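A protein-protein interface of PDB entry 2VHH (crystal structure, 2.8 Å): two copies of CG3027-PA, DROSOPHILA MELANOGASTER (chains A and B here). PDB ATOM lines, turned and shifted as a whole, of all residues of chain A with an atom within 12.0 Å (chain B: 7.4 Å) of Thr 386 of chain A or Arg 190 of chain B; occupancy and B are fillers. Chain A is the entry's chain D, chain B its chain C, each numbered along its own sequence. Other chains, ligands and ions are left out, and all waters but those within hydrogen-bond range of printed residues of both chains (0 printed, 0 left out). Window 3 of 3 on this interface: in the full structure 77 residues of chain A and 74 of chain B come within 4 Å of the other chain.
Among the printed residues, pairs that only touch across the chains: Thr 386 of chain A with Arg 190 of chain B, Ile 383 of chain A with Leu 192 of chain B and Glu 385 of chain A with Leu 192 of chain B.
No position is printed for both chains.
Hydrophobic or aromatic side chains of chain A that line the printed part of chain B: Ile 383. Printed residues of chain B that touch a printed residue of chain A: Ser 186, Ser 188, Arg 190 and Leu 192. Hydrophobic or aromatic side chains of chain B that line the printed part of chain A: Leu 192. Along chain B the printed residues that touch a printed residue of chain A span positions 186 to 192.
The side-chain hydroxyl (OG) of Ser 188 of chain B lies within hydrogen-bond range of the side-chain carboxylate (OE1) of Glu 385 of chain A (2.7 Å). The side-chain hydroxyl (OG) of Ser 186 of chain B sits at hydrogen-bond distance from the side-chain carboxylate (OE2) of Glu 385 of chain A.
The side-chain hydroxyl of Ser 186 of chain B lies close to the backbone NH of Ser 188 of chain B. OG of Ser 186 of chain B sits at hydrogen-bond distance from OD1 of Asn 187 of chain B, 3.2 Å away. The backbone carbonyl oxygen (O) of Val 184 of chain B sits at hydrogen-bond distance from the backbone NH (N) of Leu 192 of chain B (2.9 Å). N of Arg 190 of chain B lies within hydrogen-bond range of OG of Ser 188 of chain B, 3.3 Å away.
Of the printed residues of chain B, Thr 386 of chain A touches Arg 190. Printed residues of chain A within 4 Å of Arg 190 of chain B: Thr 386. No residue of chain A comes within 4 Å of Ala 156 of chain B. Ser 186 of chain B touches just one residue of chain A: Glu 385. Ser 188 of chain B touches one residue of chain A. No residue of chain A comes within 4 Å of Gly 189 of chain B. Leu 192 of chain B touches two residues of chain A. Of the printed residues of chain B, Glu 385 of chain A touches Ser 186 (2.7 Å), Ser 188 (2.7 Å) and Leu 192 (3.6 Å). Of the printed residues of chain B, Ile 383 of chain A touches Leu 192 (3.5 Å). Gly 193 of chain B touches none of the printed residues of chain A. Ile 382 of chain A touches none of the printed residues of chain B. The nearest residue of chain B that does not touch Thr 386 of chain A is Leu 192 of chain B (5.0 Å).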
ATOM      1  N   ILE A 382      -1.152 -15.198 -17.336  1.00  0.00           N
ATOM      2  CA  ILE A 382      -2.124 -14.420 -18.090  1.00  0.00           C
ATOM      3  C   ILE A 382      -2.027 -12.936 -17.776  1.00  0.00           C
ATOM      4  O   ILE A 382      -2.006 -12.543 -16.620  1.00  0.00           O
ATOM      5  CB  ILE A 382      -3.578 -14.969 -17.949  1.00  0.00           C
ATOM      6  CG1 ILE A 382      -3.641 -16.425 -18.445  1.00  0.00           C
ATOM      7  CG2 ILE A 382      -4.558 -14.094 -18.738  1.00  0.00           C
ATOM      8  CD1 ILE A 382      -5.027 -16.947 -18.776  1.00  0.00           C
ATOM      9  N   ILE A 383      -1.943 -12.130 -18.829  1.00  0.00           N
ATOM     10  CA  ILE A 383      -1.904 -10.678 -18.714  1.00  0.00           C
ATOM     11  C   ILE A 383      -3.288 -10.096 -19.036  1.00  0.00           C
ATOM     12  O   ILE A 383      -3.768 -10.209 -20.157  1.00  0.00           O
ATOM     13  CB  ILE A 383      -0.787 -10.076 -19.615  1.00  0.00           C
ATOM     14  CG1 ILE A 383       0.589 -10.602 -19.173  1.00  0.00           C
ATOM     15  CG2 ILE A 383      -0.813  -8.554 -19.572  1.00  0.00           C
ATOM     16  CD1 ILE A 383       1.791 -10.120 -20.005  1.00  0.00           C
ATOM     17  N   LYS A 384      -3.924  -9.501 -18.029  1.00  0.00           N
ATOM     18  CA  LYS A 384      -5.256  -8.916 -18.164  1.00  0.00           C
ATOM     19  C   LYS A 384      -5.157  -7.410 -18.375  1.00  0.00           C
ATOM     20  O   LYS A 384      -4.122  -6.804 -18.083  1.00  0.00           O
ATOM     21  CB  LYS A 384      -6.097  -9.190 -16.913  1.00  0.00           C
ATOM     22  CG  LYS A 384      -6.554 -10.629 -16.748  1.00  0.00           C
ATOM     23  CD  LYS A 384      -6.700 -10.993 -15.255  1.00  0.00           C
ATOM     24  CE  LYS A 384      -6.930 -12.507 -15.043  1.00  0.00           C
ATOM     25  NZ  LYS A 384      -6.629 -12.964 -13.645  1.00  0.00           N
ATOM     26  N   GLU A 385      -6.229  -6.801 -18.887  1.00  0.00           N
ATOM     27  CA  GLU A 385      -6.276  -5.340 -18.949  1.00  0.00           C
ATOM     28  C   GLU A 385      -6.519  -4.763 -17.565  1.00  0.00           C
ATOM     29  O   GLU A 385      -7.460  -5.124 -16.848  1.00  0.00           O
ATOM     30  CB  GLU A 385      -7.289  -4.794 -19.962  1.00  0.00           C
ATOM     31  CG  GLU A 385      -7.184  -3.270 -20.182  1.00  0.00           C
ATOM     32  CD  GLU A 385      -7.868  -2.790 -21.465  1.00  0.00           C
ATOM     33  OE1 GLU A 385      -7.987  -1.559 -21.651  1.00  0.00           O
ATOM     34  OE2 GLU A 385      -8.282  -3.638 -22.295  1.00  0.00           O
ATOM     35  N   THR A 386      -5.626  -3.859 -17.209  1.00  0.00           N
ATOM     36  CA  THR A 386      -5.647  -3.201 -15.931  1.00  0.00           C
ATOM     37  C   THR A 386      -6.685  -2.074 -15.970  1.00  0.00           C
ATOM     38  O   THR A 386      -7.293  -1.733 -14.949  1.00  0.00           O
ATOM     39  CB  THR A 386      -4.221  -2.692 -15.600  1.00  0.00           C
ATOM     40  OG1 THR A 386      -4.020  -2.666 -14.182  1.00  0.00           O
ATOM     41  CG2 THR A 386      -3.961  -1.316 -16.218  1.00  0.00           C
ATOM     42  N   GLU B 144       6.834   0.551 -25.130  1.00  0.00           N
ATOM     43  CA  GLU B 144       5.602   1.228 -24.735  1.00  0.00           C
ATOM     44  C   GLU B 144       5.507   2.693 -25.201  1.00  0.00           C
ATOM     45  O   GLU B 144       4.411   3.179 -25.530  1.00  0.00           O
ATOM     46  CB  GLU B 144       5.415   1.138 -23.224  1.00  0.00           C
ATOM     47  CG  GLU B 144       4.044   1.606 -22.769  1.00  0.00           C
ATOM     48  CD  GLU B 144       3.817   1.479 -21.276  1.00  0.00           C
ATOM     49  OE1 GLU B 144       4.454   0.624 -20.622  1.00  0.00           O
ATOM     50  OE2 GLU B 144       2.975   2.237 -20.758  1.00  0.00           O
ATOM     51  N   THR B 149       4.345   2.309 -31.399  1.00  0.00           N
ATOM     52  CA  THR B 149       3.256   1.947 -30.505  1.00  0.00           C
ATOM     53  C   THR B 149       2.289   3.119 -30.292  1.00  0.00           C
ATOM     54  O   THR B 149       1.084   2.910 -30.278  1.00  0.00           O
ATOM     55  CB  THR B 149       3.776   1.364 -29.156  1.00  0.00           C
ATOM     56  OG1 THR B 149       4.462   0.129 -29.401  1.00  0.00           O
ATOM     57  CG2 THR B 149       2.629   1.090 -28.182  1.00  0.00           C
ATOM     58  N   ALA B 153      -1.514   2.883 -31.331  1.00  0.00           N
ATOM     59  CA  ALA B 153      -2.506   2.915 -30.260  1.00  0.00           C
ATOM     60  C   ALA B 153      -3.685   3.834 -30.599  1.00  0.00           C
ATOM     61  O   ALA B 153      -4.816   3.563 -30.214  1.00  0.00           O
ATOM     62  CB  ALA B 153      -1.863   3.311 -28.943  1.00  0.00           C
ATOM     63  N   ALA B 156      -5.784   1.688 -32.712  1.00  0.00           N
ATOM     64  CA  ALA B 156      -6.453   0.689 -31.895  1.00  0.00           C
ATOM     65  C   ALA B 156      -7.686   1.282 -31.221  1.00  0.00           C
ATOM     66  O   ALA B 156      -8.730   0.639 -31.175  1.00  0.00           O
ATOM     67  CB  ALA B 156      -5.484   0.114 -30.861  1.00  0.00           C
ATOM     68  N   LYS B 157      -7.554   2.511 -30.721  1.00  0.00           N
ATOM     69  CA  LYS B 157      -8.636   3.216 -30.027  1.00  0.00           C
ATOM     70  C   LYS B 157      -9.740   3.561 -31.003  1.00  0.00           C
ATOM     71  O   LYS B 157     -10.903   3.280 -30.744  1.00  0.00           O
ATOM     72  CB  LYS B 157      -8.117   4.502 -29.371  1.00  0.00           C
ATOM     73  CG  LYS B 157      -8.863   4.946 -28.105  1.00  0.00           C
ATOM     74  CD  LYS B 157      -8.660   6.447 -27.855  1.00  0.00           C
ATOM     75  CE  LYS B 157      -8.374   6.789 -26.385  1.00  0.00           C
ATOM     76  NZ  LYS B 157      -6.910   6.694 -26.041  1.00  0.00           N
ATOM     77  N   VAL B 184       1.452  -5.931 -27.472  1.00  0.00           N
ATOM     78  CA  VAL B 184       0.000  -6.040 -27.565  1.00  0.00           C
ATOM     79  C   VAL B 184      -0.643  -4.758 -27.079  1.00  0.00           C
ATOM     80  O   VAL B 184      -0.434  -4.324 -25.941  1.00  0.00           O
ATOM     81  CB  VAL B 184      -0.555  -7.251 -26.775  1.00  0.00           C
ATOM     82  CG1 VAL B 184      -2.083  -7.284 -26.820  1.00  0.00           C
ATOM     83  CG2 VAL B 184      -0.006  -8.541 -27.345  1.00  0.00           C
ATOM     84  N   ILE B 185      -1.420  -4.153 -27.968  1.00  0.00           N
ATOM     85  CA  ILE B 185      -2.168  -2.937 -27.663  1.00  0.00           C
ATOM     86  C   ILE B 185      -3.644  -3.301 -27.605  1.00  0.00           C
ATOM     87  O   ILE B 185      -4.165  -3.936 -28.512  1.00  0.00           O
ATOM     88  CB  ILE B 185      -1.925  -1.844 -28.725  1.00  0.00           C
ATOM     89  CG1 ILE B 185      -0.436  -1.522 -28.831  1.00  0.00           C
ATOM     90  CG2 ILE B 185      -2.652  -0.580 -28.355  1.00  0.00           C
ATOM     91  CD1 ILE B 185      -0.008  -0.959 -30.178  1.00  0.00           C
ATOM     92  N   SER B 186      -4.300  -2.910 -26.520  1.00  0.00           N
ATOM     93  CA  SER B 186      -5.716  -3.178 -26.321  1.00  0.00           C
ATOM     94  C   SER B 186      -6.594  -2.339 -27.247  1.00  0.00           C
ATOM     95  O   SER B 186      -6.167  -1.283 -27.735  1.00  0.00           O
ATOM     96  CB  SER B 186      -6.093  -2.884 -24.877  1.00  0.00           C
ATOM     97  OG  SER B 186      -7.498  -2.878 -24.713  1.00  0.00           O
ATOM     98  N   ASN B 187      -7.824  -2.808 -27.472  1.00  0.00           N
ATOM     99  CA  ASN B 187      -8.819  -2.048 -28.246  1.00  0.00           C
ATOM    100  C   ASN B 187      -9.267  -0.743 -27.573  1.00  0.00           C
ATOM    101  O   ASN B 187      -9.953   0.070 -28.183  1.00  0.00           O
ATOM    102  CB  ASN B 187     -10.041  -2.906 -28.593  1.00  0.00           C
ATOM    103  CG  ASN B 187     -10.661  -3.551 -27.384  1.00  0.00           C
ATOM    104  OD1 ASN B 187      -9.962  -3.925 -26.455  1.00  0.00           O
ATOM    105  ND2 ASN B 187     -11.978  -3.701 -27.395  1.00  0.00           N
ATOM    106  N   SER B 188      -8.876  -0.549 -26.321  1.00  0.00           N
ATOM    107  CA  SER B 188      -9.116   0.708 -25.634  1.00  0.00           C
ATOM    108  C   SER B 188      -8.054   1.735 -26.024  1.00  0.00           C
ATOM    109  O   SER B 188      -8.227   2.932 -25.810  1.00  0.00           O
ATOM    110  CB  SER B 188      -9.142   0.509 -24.108  1.00  0.00           C
ATOM    111  OG  SER B 188      -7.836   0.381 -23.578  1.00  0.00           O
ATOM    112  N   GLY B 189      -6.955   1.257 -26.598  1.00  0.00           N
ATOM    113  CA  GLY B 189      -5.835   2.120 -26.960  1.00  0.00           C
ATOM    114  C   GLY B 189      -4.676   2.023 -25.980  1.00  0.00           C
ATOM    115  O   GLY B 189      -3.579   2.515 -26.256  1.00  0.00           O
ATOM    116  N   ARG B 190      -4.916   1.387 -24.835  1.00  0.00           N
ATOM    117  CA  ARG B 190      -3.897   1.264 -23.790  1.00  0.00           C
ATOM    118  C   ARG B 190      -2.944   0.114 -24.070  1.00  0.00           C
ATOM    119  O   ARG B 190      -3.333  -0.895 -24.655  1.00  0.00           O
ATOM    120  CB  ARG B 190      -4.535   1.138 -22.398  1.00  0.00           C
ATOM    121  CG  ARG B 190      -5.439   2.331 -22.056  1.00  0.00           C
ATOM    122  CD  ARG B 190      -5.492   2.667 -20.571  1.00  0.00           C
ATOM    123  NE  ARG B 190      -6.287   1.717 -19.778  1.00  0.00           N
ATOM    124  CZ  ARG B 190      -5.787   0.932 -18.816  1.00  0.00           C
ATOM    125  NH1 ARG B 190      -4.491   0.967 -18.520  1.00  0.00           N
ATOM    126  NH2 ARG B 190      -6.585   0.119 -18.130  1.00  0.00           N
ATOM    127  N   TYR B 191      -1.686   0.296 -23.680  1.00  0.00           N
ATOM    128  CA  TYR B 191      -0.667  -0.719 -23.851  1.00  0.00           C
ATOM    129  C   TYR B 191      -0.944  -1.866 -22.888  1.00  0.00           C
ATOM    130  O   TYR B 191      -1.188  -1.633 -21.709  1.00  0.00           O
ATOM    131  CB  TYR B 191       0.689  -0.081 -23.599  1.00  0.00           C
ATOM    132  CG  TYR B 191       1.837  -1.018 -23.337  1.00  0.00           C
ATOM    133  CD1 TYR B 191       2.626  -1.494 -24.386  1.00  0.00           C
ATOM    134  CD2 TYR B 191       2.170  -1.389 -22.023  1.00  0.00           C
ATOM    135  CE1 TYR B 191       3.707  -2.339 -24.137  1.00  0.00           C
ATOM    136  CE2 TYR B 191       3.245  -2.232 -21.761  1.00  0.00           C
ATOM    137  CZ  TYR B 191       4.010  -2.702 -22.820  1.00  0.00           C
ATOM    138  OH  TYR B 191       5.078  -3.534 -22.565  1.00  0.00           O
ATOM    139  N   LEU B 192      -0.939  -3.097 -23.392  1.00  0.00           N
ATOM    140  CA  LEU B 192      -1.229  -4.259 -22.546  1.00  0.00           C
ATOM    141  C   LEU B 192       0.010  -4.904 -21.966  1.00  0.00           C
ATOM    142  O   LEU B 192       0.000  -5.333 -20.814  1.00  0.00           O
ATOM    143  CB  LEU B 192      -2.022  -5.332 -23.294  1.00  0.00           C
ATOM    144  CG  LEU B 192      -3.540  -5.277 -23.191  1.00  0.00           C
ATOM    145  CD1 LEU B 192      -4.136  -6.594 -23.677  1.00  0.00           C
ATOM    146  CD2 LEU B 192      -3.979  -4.969 -21.754  1.00  0.00           C
ATOM    147  N   GLY B 193       1.062  -4.996 -22.774  1.00  0.00           N
ATOM    148  CA  GLY B 193       2.266  -5.675 -22.362  1.00  0.00           C
ATOM    149  C   GLY B 193       3.090  -6.096 -23.547  1.00  0.00           C
ATOM    150  O   GLY B 193       2.781  -5.741 -24.682  1.00  0.00           O
